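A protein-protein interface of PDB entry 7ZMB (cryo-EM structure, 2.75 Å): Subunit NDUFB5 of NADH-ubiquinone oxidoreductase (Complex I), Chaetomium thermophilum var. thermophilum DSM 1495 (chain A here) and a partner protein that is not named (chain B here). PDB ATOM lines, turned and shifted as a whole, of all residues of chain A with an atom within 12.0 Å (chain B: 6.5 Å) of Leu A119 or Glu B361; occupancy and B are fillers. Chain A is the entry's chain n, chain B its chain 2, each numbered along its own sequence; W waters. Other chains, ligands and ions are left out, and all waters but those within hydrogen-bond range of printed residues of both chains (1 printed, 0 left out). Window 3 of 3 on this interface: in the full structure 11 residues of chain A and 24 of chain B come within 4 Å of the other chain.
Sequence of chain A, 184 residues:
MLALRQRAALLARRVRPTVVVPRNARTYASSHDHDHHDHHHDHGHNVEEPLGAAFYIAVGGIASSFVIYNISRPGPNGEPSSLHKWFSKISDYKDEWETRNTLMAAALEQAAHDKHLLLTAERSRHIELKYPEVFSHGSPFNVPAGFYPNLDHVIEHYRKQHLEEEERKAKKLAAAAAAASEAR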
ATOM      1  N   GLN A 110      12.851   5.889  -2.033  1.00  0.00           N
ATOM      2  CA  GLN A 110      11.420   6.150  -2.086  1.00  0.00           C
ATOM      3  C   GLN A 110      10.813   5.613  -3.372  1.00  0.00           C
ATOM      4  O   GLN A 110       9.740   4.999  -3.349  1.00  0.00           O
ATOM      5  CB  GLN A 110      11.150   7.646  -1.941  1.00  0.00           C
ATOM      6  CG  GLN A 110       9.714   7.964  -1.585  1.00  0.00           C
ATOM      7  CD  GLN A 110       9.201   7.118  -0.436  1.00  0.00           C
ATOM      8  OE1 GLN A 110       8.559   6.089  -0.645  1.00  0.00           O
ATOM      9  NE2 GLN A 110       9.482   7.551   0.788  1.00  0.00           N
ATOM     10  N   ALA A 111      11.500   5.804  -4.497  1.00  0.00           N
ATOM     11  CA  ALA A 111      11.021   5.250  -5.756  1.00  0.00           C
ATOM     12  C   ALA A 111      10.947   3.733  -5.696  1.00  0.00           C
ATOM     13  O   ALA A 111       9.990   3.132  -6.190  1.00  0.00           O
ATOM     14  CB  ALA A 111      11.919   5.699  -6.906  1.00  0.00           C
ATOM     15  N   ALA A 112      11.946   3.097  -5.083  1.00  0.00           N
ATOM     16  CA  ALA A 112      11.941   1.641  -4.972  1.00  0.00           C
ATOM     17  C   ALA A 112      10.754   1.155  -4.153  1.00  0.00           C
ATOM     18  O   ALA A 112      10.175   0.106  -4.448  1.00  0.00           O
ATOM     19  CB  ALA A 112      13.250   1.155  -4.356  1.00  0.00           C
ATOM     20  N   HIS A 113      10.381   1.916  -3.125  1.00  0.00           N
ATOM     21  CA  HIS A 113       9.213   1.551  -2.284  1.00  0.00           C
ATOM     22  C   HIS A 113       7.925   1.719  -3.091  1.00  0.00           C
ATOM     23  O   HIS A 113       7.029   0.878  -2.946  1.00  0.00           O
ATOM     24  CB  HIS A 113       9.185   2.397  -1.007  1.00  0.00           C
ATOM     25  CG  HIS A 113       7.886   2.329  -0.279  1.00  0.00           C
ATOM     26  ND1 HIS A 113       7.488   1.206   0.417  1.00  0.00           N
ATOM     27  CD2 HIS A 113       6.890   3.231  -0.147  1.00  0.00           C
ATOM     28  CE1 HIS A 113       6.304   1.420   0.951  1.00  0.00           C
ATOM     29  NE2 HIS A 113       5.915   2.656   0.620  1.00  0.00           N
ATOM     30  N   ASP A 114       7.839   2.783  -3.888  1.00  0.00           N
ATOM     31  CA  ASP A 114       6.637   3.004  -4.687  1.00  0.00           C
ATOM     32  C   ASP A 114       6.431   1.874  -5.680  1.00  0.00           C
ATOM     33  O   ASP A 114       5.321   1.353  -5.824  1.00  0.00           O
ATOM     34  CB  ASP A 114       6.721   4.346  -5.411  1.00  0.00           C
ATOM     35  CG  ASP A 114       7.040   5.494  -4.476  1.00  0.00           C
ATOM     36  OD1 ASP A 114       6.674   5.413  -3.285  1.00  0.00           O
ATOM     37  OD2 ASP A 114       7.660   6.478  -4.932  1.00  0.00           O
ATOM     38  N   LYS A 115       7.502   1.472  -6.366  1.00  0.00           N
ATOM     39  CA  LYS A 115       7.412   0.348  -7.287  1.00  0.00           C
ATOM     40  C   LYS A 115       7.037  -0.922  -6.547  1.00  0.00           C
ATOM     41  O   LYS A 115       6.220  -1.713  -7.029  1.00  0.00           O
ATOM     42  CB  LYS A 115       8.736   0.180  -8.032  1.00  0.00           C
ATOM     43  CG  LYS A 115       8.870  -1.107  -8.832  1.00  0.00           C
ATOM     44  CD  LYS A 115      10.191  -1.145  -9.589  1.00  0.00           C
ATOM     45  CE  LYS A 115      10.605  -2.568  -9.934  1.00  0.00           C
ATOM     46  NZ  LYS A 115      11.398  -3.213  -8.845  1.00  0.00           N
ATOM     47  N   HIS A 116       7.603  -1.120  -5.357  1.00  0.00           N
ATOM     48  CA  HIS A 116       7.261  -2.284  -4.546  1.00  0.00           C
ATOM     49  C   HIS A 116       5.779  -2.291  -4.189  1.00  0.00           C
ATOM     50  O   HIS A 116       5.129  -3.338  -4.225  1.00  0.00           O
ATOM     51  CB  HIS A 116       8.145  -2.298  -3.301  1.00  0.00           C
ATOM     52  CG  HIS A 116       7.665  -3.198  -2.208  1.00  0.00           C
ATOM     53  ND1 HIS A 116       7.618  -2.799  -0.890  1.00  0.00           N
ATOM     54  CD2 HIS A 116       7.231  -4.479  -2.229  1.00  0.00           C
ATOM     55  CE1 HIS A 116       7.170  -3.793  -0.148  1.00  0.00           C
ATOM     56  NE2 HIS A 116       6.925  -4.823  -0.937  1.00  0.00           N
ATOM     57  N   LEU A 117       5.226  -1.122  -3.868  1.00  0.00           N
ATOM     58  CA  LEU A 117       3.791  -0.994  -3.638  1.00  0.00           C
ATOM     59  C   LEU A 117       2.976  -1.349  -4.877  1.00  0.00           C
ATOM     60  O   LEU A 117       1.967  -2.055  -4.784  1.00  0.00           O
ATOM     61  CB  LEU A 117       3.479   0.435  -3.201  1.00  0.00           C
ATOM     62  CG  LEU A 117       2.352   0.758  -2.223  1.00  0.00           C
ATOM     63  CD1 LEU A 117       2.502   0.017  -0.936  1.00  0.00           C
ATOM     64  CD2 LEU A 117       2.332   2.252  -1.972  1.00  0.00           C
ATOM     65  N   LEU A 118       3.267  -0.702  -6.002  1.00  0.00           N
ATOM     66  CA  LEU A 118       2.458  -0.895  -7.230  1.00  0.00           C
ATOM     67  C   LEU A 118       2.579  -2.331  -7.764  1.00  0.00           C
ATOM     68  O   LEU A 118       1.547  -2.891  -8.164  1.00  0.00           O
ATOM     69  CB  LEU A 118       2.871   0.157  -8.264  1.00  0.00           C
ATOM     70  CG  LEU A 118       2.571   1.610  -7.908  1.00  0.00           C
ATOM     71  CD1 LEU A 118       3.541   2.542  -8.613  1.00  0.00           C
ATOM     72  CD2 LEU A 118       1.139   1.973  -8.260  1.00  0.00           C
ATOM     73  N   LEU A 119       3.784  -2.887  -7.827  1.00  0.00           N
ATOM     74  CA  LEU A 119       3.987  -4.268  -8.352  1.00  0.00           C
ATOM     75  C   LEU A 119       3.309  -5.318  -7.468  1.00  0.00           C
ATOM     76  O   LEU A 119       2.810  -6.303  -8.025  1.00  0.00           O
ATOM     77  CB  LEU A 119       5.477  -4.561  -8.530  1.00  0.00           C
ATOM     78  CG  LEU A 119       5.923  -4.782  -9.974  1.00  0.00           C
ATOM     79  CD1 LEU A 119       5.707  -3.525 -10.800  1.00  0.00           C
ATOM     80  CD2 LEU A 119       7.380  -5.212 -10.029  1.00  0.00           C
ATOM     81  N   THR A 120       3.327  -5.144  -6.147  1.00  0.00           N
ATOM     82  CA  THR A 120       2.795  -6.198  -5.248  1.00  0.00           C
ATOM     83  C   THR A 120       1.352  -5.922  -4.838  1.00  0.00           C
ATOM     84  O   THR A 120       0.916  -6.536  -3.855  1.00  0.00           O
ATOM     85  CB  THR A 120       3.664  -6.356  -3.998  1.00  0.00           C
ATOM     86  OG1 THR A 120       3.536  -5.155  -3.239  1.00  0.00           O
ATOM     87  CG2 THR A 120       5.117  -6.637  -4.313  1.00  0.00           C
ATOM     88  N   ALA A 121       0.632  -5.073  -5.574  1.00  0.00           N
ATOM     89  CA  ALA A 121      -0.782  -4.761  -5.263  1.00  0.00           C
ATOM     90  C   ALA A 121      -1.648  -5.995  -5.495  1.00  0.00           C
ATOM     91  O   ALA A 121      -1.441  -6.686  -6.497  1.00  0.00           O
ATOM     92  CB  ALA A 121      -1.249  -3.615  -6.102  1.00  0.00           C
ATOM     93  N   GLU A 122      -2.602  -6.243  -4.602  1.00  0.00           N
ATOM     94  CA  GLU A 122      -3.445  -7.463  -4.697  1.00  0.00           C
ATOM     95  C   GLU A 122      -4.310  -7.449  -5.957  1.00  0.00           C
ATOM     96  O   GLU A 122      -4.819  -6.373  -6.314  1.00  0.00           O
ATOM     97  CB  GLU A 122      -4.336  -7.575  -3.462  1.00  0.00           C
ATOM     98  CG  GLU A 122      -3.556  -7.574  -2.160  1.00  0.00           C
ATOM     99  CD  GLU A 122      -4.395  -7.808  -0.916  1.00  0.00           C
ATOM    100  OE1 GLU A 122      -3.927  -7.456   0.185  1.00  0.00           O
ATOM    101  OE2 GLU A 122      -5.512  -8.345  -1.051  1.00  0.00           O
ATOM    102  N   ARG A 123      -4.460  -8.606  -6.602  1.00  0.00           N
ATOM    103  CA  ARG A 123      -5.378  -8.724  -7.761  1.00  0.00           C
ATOM    104  C   ARG A 123      -6.769  -8.900  -7.169  1.00  0.00           C
ATOM    105  O   ARG A 123      -6.891  -9.653  -6.185  1.00  0.00           O
ATOM    106  CB  ARG A 123      -5.031  -9.986  -8.555  1.00  0.00           C
ATOM    107  CG  ARG A 123      -5.912 -10.298  -9.752  1.00  0.00           C
ATOM    108  CD  ARG A 123      -5.571 -11.713 -10.167  1.00  0.00           C
ATOM    109  NE  ARG A 123      -5.918 -12.044 -11.538  1.00  0.00           N
ATOM    110  CZ  ARG A 123      -5.027 -12.263 -12.493  1.00  0.00           C
ATOM    111  NH1 ARG A 123      -3.737 -12.199 -12.221  1.00  0.00           N
ATOM    112  NH2 ARG A 123      -5.430 -12.557 -13.713  1.00  0.00           N
ATOM    113  N   SER A 124      -7.770  -8.238  -7.746  1.00  0.00           N
ATOM    114  CA  SER A 124      -9.155  -8.425  -7.270  1.00  0.00           C
ATOM    115  C   SER A 124      -9.764  -9.695  -7.839  1.00  0.00           C
ATOM    116  O   SER A 124      -9.558  -9.953  -9.026  1.00  0.00           O
ATOM    117  CB  SER A 124     -10.020  -7.265  -7.612  1.00  0.00           C
ATOM    118  OG  SER A 124     -11.345  -7.475  -7.149  1.00  0.00           O
ATOM    119  N   SER B 359       0.227 -11.051 -14.219  1.00  0.00           N
ATOM    120  CA  SER B 359       0.675 -10.326 -13.022  1.00  0.00           C
ATOM    121  C   SER B 359       0.824  -8.876 -13.450  1.00  0.00           C
ATOM    122  O   SER B 359       0.861  -8.631 -14.653  1.00  0.00           O
ATOM    123  CB  SER B 359       1.983 -10.890 -12.562  1.00  0.00           C
ATOM    124  OG  SER B 359       3.048 -10.459 -13.391  1.00  0.00           O
ATOM    125  N   ILE B 360       0.811  -7.960 -12.492  1.00  0.00           N
ATOM    126  CA  ILE B 360       0.981  -6.518 -12.814  1.00  0.00           C
ATOM    127  C   ILE B 360       2.244  -6.358 -13.661  1.00  0.00           C
ATOM    128  O   ILE B 360       2.138  -5.800 -14.761  1.00  0.00           O
ATOM    129  CB  ILE B 360       0.989  -5.669 -11.526  1.00  0.00           C
ATOM    130  CG1 ILE B 360      -0.368  -5.723 -10.822  1.00  0.00           C
ATOM    131  CG2 ILE B 360       1.436  -4.242 -11.800  1.00  0.00           C
ATOM    132  CD1 ILE B 360      -0.288  -5.523  -9.337  1.00  0.00           C
ATOM    133  N   GLU B 361       3.379  -6.875 -13.192  1.00  0.00           N
ATOM    134  CA  GLU B 361       4.658  -6.667 -13.921  1.00  0.00           C
ATOM    135  C   GLU B 361       4.563  -7.287 -15.323  1.00  0.00           C
ATOM    136  O   GLU B 361       5.024  -6.631 -16.275  1.00  0.00           O
ATOM    137  CB  GLU B 361       5.866  -7.162 -13.126  1.00  0.00           C
ATOM    138  CG  GLU B 361       7.179  -6.676 -13.709  1.00  0.00           C
ATOM    139  CD  GLU B 361       8.453  -7.196 -13.069  1.00  0.00           C
ATOM    140  OE1 GLU B 361       8.381  -8.181 -12.316  1.00  0.00           O
ATOM    141  OE2 GLU B 361       9.517  -6.605 -13.329  1.00  0.00           O
ATOM    142  N   SER B 362       3.940  -8.458 -15.459  1.00  0.00           N
ATOM    143  CA  SER B 362       3.905  -9.125 -16.784  1.00  0.00           C
ATOM    144  C   SER B 362       2.886  -8.468 -17.713  1.00  0.00           C
ATOM    145  O   SER B 362       3.032  -8.630 -18.922  1.00  0.00           O
ATOM    146  CB  SER B 362       3.575 -10.568 -16.639  1.00  0.00           C
ATOM    147  OG  SER B 362       2.199 -10.722 -16.349  1.00  0.00           O
ATOM    148  N   THR B 363       1.907  -7.755 -17.159  1.00  0.00           N
ATOM    149  CA  THR B 363       0.858  -7.101 -17.974  1.00  0.00           C
ATOM    150  C   THR B 363       1.476  -5.796 -18.452  1.00  0.00           C
ATOM    151  O   THR B 363       1.237  -5.434 -19.615  1.00  0.00           O
ATOM    152  CB  THR B 363      -0.471  -7.022 -17.205  1.00  0.00           C
ATOM    153  OG1 THR B 363      -0.796  -8.345 -16.781  1.00  0.00           O
ATOM    154  CG2 THR B 363      -1.609  -6.471 -18.036  1.00  0.00           C
ATOM    155  N   GLN B 364       2.230  -5.117 -17.587  1.00  0.00           N
ATOM    156  CA  GLN B 364       3.000  -3.974 -18.074  1.00  0.00           C
ATOM    157  C   GLN B 364       3.939  -4.407 -19.187  1.00  0.00           C
ATOM    158  O   GLN B 364       4.020  -3.760 -20.235  1.00  0.00           O
ATOM    159  CB  GLN B 364       3.805  -3.340 -16.940  1.00  0.00           C
ATOM    160  CG  GLN B 364       3.015  -2.814 -15.797  1.00  0.00           C
ATOM    161  CD  GLN B 364       3.889  -2.430 -14.633  1.00  0.00           C
ATOM    162  OE1 GLN B 364       3.787  -1.327 -14.109  1.00  0.00           O
ATOM    163  NE2 GLN B 364       4.755  -3.340 -14.215  1.00  0.00           N
ATOM    164  N   ALA B 365       4.651  -5.514 -18.975  1.00  0.00           N
ATOM    165  CA  ALA B 365       5.589  -6.010 -19.973  1.00  0.00           C
ATOM    166  C   ALA B 365       4.877  -6.397 -21.259  1.00  0.00           C
ATOM    167  O   ALA B 365       5.353  -6.092 -22.355  1.00  0.00           O
ATOM    168  CB  ALA B 365       6.369  -7.199 -19.413  1.00  0.00           C
ATOM    169  N   PHE B 366       3.734  -7.072 -21.144  1.00  0.00           N
ATOM    170  CA  PHE B 366       2.995  -7.471 -22.333  1.00  0.00           C
ATOM    171  C   PHE B 366       2.520  -6.258 -23.123  1.00  0.00           C
ATOM    172  O   PHE B 366       2.581  -6.248 -24.356  1.00  0.00           O
ATOM    173  CB  PHE B 366       1.813  -8.350 -21.939  1.00  0.00           C
ATOM    174  CG  PHE B 366       0.766  -8.468 -23.006  1.00  0.00           C
ATOM    175  CD1 PHE B 366       0.921  -9.358 -24.049  1.00  0.00           C
ATOM    176  CD2 PHE B 366      -0.379  -7.694 -22.958  1.00  0.00           C
ATOM    177  CE1 PHE B 366      -0.044  -9.467 -25.019  1.00  0.00           C
ATOM    178  CE2 PHE B 366      -1.337  -7.800 -23.928  1.00  0.00           C
ATOM    179  CZ  PHE B 366      -1.172  -8.687 -24.958  1.00  0.00           C
ATOM    180  N   GLN B 452      13.690  -7.399 -21.678  1.00  0.00           N
ATOM    181  CA  GLN B 452      14.090  -7.394 -20.249  1.00  0.00           C
ATOM    182  C   GLN B 452      12.853  -7.321 -19.346  1.00  0.00           C
ATOM    183  O   GLN B 452      12.851  -7.996 -18.311  1.00  0.00           O
ATOM    184  CB  GLN B 452      15.093  -6.260 -20.033  1.00  0.00           C
ATOM    185  CG  GLN B 452      15.411  -5.947 -18.579  1.00  0.00           C
ATOM    186  CD  GLN B 452      14.548  -4.835 -18.035  1.00  0.00           C
ATOM    187  OE1 GLN B 452      14.041  -3.997 -18.776  1.00  0.00           O
ATOM    188  NE2 GLN B 452      14.368  -4.826 -16.725  1.00  0.00           N
ATOM    189  N   MET B 453      11.850  -6.527 -19.717  1.00  0.00           N
ATOM    190  CA  MET B 453      10.638  -6.353 -18.880  1.00  0.00           C
ATOM    191  C   MET B 453       9.877  -7.673 -18.772  1.00  0.00           C
ATOM    192  O   MET B 453       9.316  -7.936 -17.699  1.00  0.00           O
ATOM    193  CB  MET B 453       9.734  -5.236 -19.408  1.00  0.00           C
ATOM    194  CG  MET B 453      10.314  -3.855 -19.199  1.00  0.00           C
ATOM    195  SD  MET B 453       9.419  -2.566 -20.087  1.00  0.00           S
ATOM    196  CE  MET B 453       7.768  -2.815 -19.438  1.00  0.00           C
ATOM    197  N   VAL B 454       9.923  -8.487 -19.820  1.00  0.00           N
ATOM    198  CA  VAL B 454       9.144  -9.755 -19.875  1.00  0.00           C
ATOM    199  C   VAL B 454       9.975 -10.790 -19.141  1.00  0.00           C
ATOM    200  O   VAL B 454       9.377 -11.608 -18.428  1.00  0.00           O
ATOM    201  CB  VAL B 454       8.863 -10.170 -21.333  1.00  0.00           C
ATOM    202  CG1 VAL B 454       8.348 -11.593 -21.455  1.00  0.00           C
ATOM    203  CG2 VAL B 454       7.941  -9.195 -22.046  1.00  0.00           C
ATOM    204  N   LEU B 455      11.297 -10.708 -19.246  1.00  0.00           N
ATOM    205  CA  LEU B 455      12.140 -11.612 -18.471  1.00  0.00           C
ATOM    206  C   LEU B 455      12.050 -11.320 -16.981  1.00  0.00           C
ATOM    207  O   LEU B 455      12.040 -12.245 -16.166  1.00  0.00           O
ATOM    208  CB  LEU B 455      13.586 -11.514 -18.945  1.00  0.00           C
ATOM    209  CG  LEU B 455      13.900 -12.057 -20.335  1.00  0.00           C
ATOM    210  CD1 LEU B 455      15.318 -11.688 -20.719  1.00  0.00           C
ATOM    211  CD2 LEU B 455      13.687 -13.558 -20.406  1.00  0.00           C
ATOM    212  N   SER B 456      12.003 -10.059 -16.606  1.00  0.00           N
ATOM    213  CA  SER B 456      11.907  -9.668 -15.176  1.00  0.00           C
ATOM    214  C   SER B 456      10.607 -10.196 -14.579  1.00  0.00           C
ATOM    215  O   SER B 456      10.642 -10.691 -13.446  1.00  0.00           O
ATOM    216  CB  SER B 456      12.002  -8.176 -15.031  1.00  0.00           C
ATOM    217  OG  SER B 456      13.258  -7.790 -14.500  1.00  0.00           O
ATOM    218  N   ALA B 457       9.501 -10.081 -15.328  1.00  0.00           N
ATOM    219  CA  ALA B 457       8.184 -10.522 -14.826  1.00  0.00           C
ATOM    220  C   ALA B 457       8.163 -12.036 -14.661  1.00  0.00           C
ATOM    221  O   ALA B 457       7.677 -12.513 -13.623  1.00  0.00           O
ATOM    222  CB  ALA B 457       7.131 -10.070 -15.789  1.00  0.00           C
ATOM    223  N   ALA B 458       8.680 -12.753 -15.655  1.00  0.00           N
ATOM    224  CA  ALA B 458       8.670 -14.229 -15.623  1.00  0.00           C
ATOM    225  C   ALA B 458       9.575 -14.733 -14.502  1.00  0.00           C
ATOM    226  O   ALA B 458       9.182 -15.685 -13.815  1.00  0.00           O
ATOM    227  CB  ALA B 458       9.067 -14.750 -16.978  1.00  0.00           C
ATOM    228  N   ASP B 460      10.289 -13.192 -11.728  1.00  0.00           N
ATOM    229  CA  ASP B 460       9.590 -12.903 -10.453  1.00  0.00           C
ATOM    230  C   ASP B 460       8.509 -13.954 -10.198  1.00  0.00           C
ATOM    231  O   ASP B 460       8.350 -14.352  -9.035  1.00  0.00           O
ATOM    232  CB  ASP B 460       9.032 -11.486 -10.406  1.00  0.00           C
ATOM    233  CG  ASP B 460       9.176 -10.828  -9.046  1.00  0.00           C
ATOM    234  OD1 ASP B 460       9.598 -11.522  -8.102  1.00  0.00           O
ATOM    235  OD2 ASP B 460       8.870  -9.626  -8.942  1.00  0.00           O
ATOM    236  N   ASN B 461       7.811 -14.399 -11.239  1.00  0.00           N
ATOM    237  CA  ASN B 461       6.676 -15.317 -10.978  1.00  0.00           C
ATOM    238  C   ASN B 461       7.043 -16.802 -11.053  1.00  0.00           C
ATOM    239  O   ASN B 461       6.113 -17.608 -11.131  1.00  0.00           O
ATOM    240  CB  ASN B 461       5.401 -14.931 -11.729  1.00  0.00           C
ATOM    241  CG  ASN B 461       4.517 -14.001 -10.929  1.00  0.00           C
ATOM    242  OD1 ASN B 461       5.005 -13.226 -10.111  1.00  0.00           O
ATOM    243  ND2 ASN B 461       3.217 -14.068 -11.157  1.00  0.00           N
ATOM    244  N   VAL B 565      -2.532  -1.082 -16.186  1.00  0.00           N
ATOM    245  CA  VAL B 565      -2.466  -2.331 -15.377  1.00  0.00           C
ATOM    246  C   VAL B 565      -3.060  -2.101 -13.991  1.00  0.00           C
ATOM    247  O   VAL B 565      -3.770  -2.988 -13.511  1.00  0.00           O
ATOM    248  CB  VAL B 565      -1.042  -2.901 -15.345  1.00  0.00           C
ATOM    249  CG1 VAL B 565      -0.967  -4.180 -14.534  1.00  0.00           C
ATOM    250  CG2 VAL B 565      -0.556  -3.153 -16.761  1.00  0.00           C
ATOM    251  N   GLN B 566      -2.799  -0.943 -13.398  1.00  0.00           N
ATOM    252  CA  GLN B 566      -3.391  -0.621 -12.082  1.00  0.00           C
ATOM    253  C   GLN B 566      -4.914  -0.598 -12.205  1.00  0.00           C
ATOM    254  O   GLN B 566      -5.529  -1.313 -11.446  1.00  0.00           O
ATOM    255  CB  GLN B 566      -2.821   0.684 -11.536  1.00  0.00           C
ATOM    256  CG  GLN B 566      -1.365   0.590 -11.111  1.00  0.00           C
ATOM    257  CD  GLN B 566      -1.144  -0.486 -10.079  1.00  0.00           C
ATOM    258  OE1 GLN B 566      -1.792  -0.512  -9.039  1.00  0.00           O
ATOM    259  NE2 GLN B 566      -0.211  -1.379 -10.354  1.00  0.00           N
ATOM    260  N   PHE B 569      -6.236  -4.324 -12.530  1.00  0.00           N
ATOM    261  CA  PHE B 569      -6.011  -5.210 -11.364  1.00  0.00           C
ATOM    262  C   PHE B 569      -6.502  -4.593 -10.056  1.00  0.00           C
ATOM    263  O   PHE B 569      -6.264  -5.221  -9.029  1.00  0.00           O
ATOM    264  CB  PHE B 569      -4.504  -5.449 -11.233  1.00  0.00           C
ATOM    265  CG  PHE B 569      -3.899  -6.591 -12.004  1.00  0.00           C
ATOM    266  CD1 PHE B 569      -3.644  -6.482 -13.360  1.00  0.00           C
ATOM    267  CD2 PHE B 569      -3.518  -7.752 -11.355  1.00  0.00           C
ATOM    268  CE1 PHE B 569      -3.061  -7.527 -14.057  1.00  0.00           C
ATOM    269  CE2 PHE B 569      -2.931  -8.796 -12.055  1.00  0.00           C
ATOM    270  CZ  PHE B 569      -2.710  -8.683 -13.406  1.00  0.00           C
HETATM  271  O   HOH W   1       3.478  -8.012 -10.349  1.00  0.00           O
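The backbone carbonyl oxygen (O) of Glu A122 sits close to the backbone carbonyl oxygen (O) of Phe B569. The backbone carbonyl oxygen of Leu A118 sits at hydrogen-bond distance from the side-chain amide nitrogen of Gln B566 (3.2 Å).
Printed residues of chain B that touch a printed residue of chain A: Ile B360, Glu B361, Gln B364, Gln B566 and Phe B569. Hydrophobic or aromatic side chains of chain A that line the printed part of chain B: Leu A118, Leu A119 and Ala A121.
Water W1 lies within hydrogen-bond range of O of Leu A119 (3.0 Å), N of Glu B361 (3.1 Å) and N of Ile B360 (3.4 Å).
Printed residues of chain B within 4 Å of Leu A118: Ile B360 (3.4 Å) and Gln B566 (3.2 Å). Thr A120 touches none of the printed residues of chain B. Printed residues of chain B within 4 Å of Ala A121: Ile B360 (3.3 Å). Printed residues of chain B within 4 Å of Glu A122: Phe B569. Printed residues of chain A within 4 Å of Ile B360: Leu A118 (3.4 Å), Leu A119 (3.5 Å) and Ala A121 (3.3 Å). Glu B361 touches one residue of chain A. No residue of chain A comes within 4 Å of Ser B362. No residue of chain A comes within 4 Å of Thr B363. No residue of chain A comes within 4 Å of Ala B365. Gln B452 touches none of the printed residues of chain A. No residue of chain A comes within 4 Å of Met B453. No residue of chain A comes within 4 Å of Val B454. No residue of chain A comes within 4 Å of Ser B456. No residue of chain A comes within 4 Å of Ala B457. No residue of chain A comes within 4 Å of Asp B460. The nearest residue of chain B that does not touch Leu A119 is Asp B460 (4.8 Å). The nearest residue of chain A that does not touch Glu B361 is Lys A115 (5.4 Å).
Among the printed residues, pairs that only touch across the chains: Ala A121 with Ile B360 (3.3 Å), Leu A118 with Ile B360 (3.4 Å), Leu A119 with Ile B360 (3.5 Å), Arg A123 with Phe B569 (3.5 Å), Leu A119 with Gln B364 (3.6 Å), Ser A124 with Phe B569 (3.6 Å) and Leu A119 with Glu B361 (3.8 Å).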
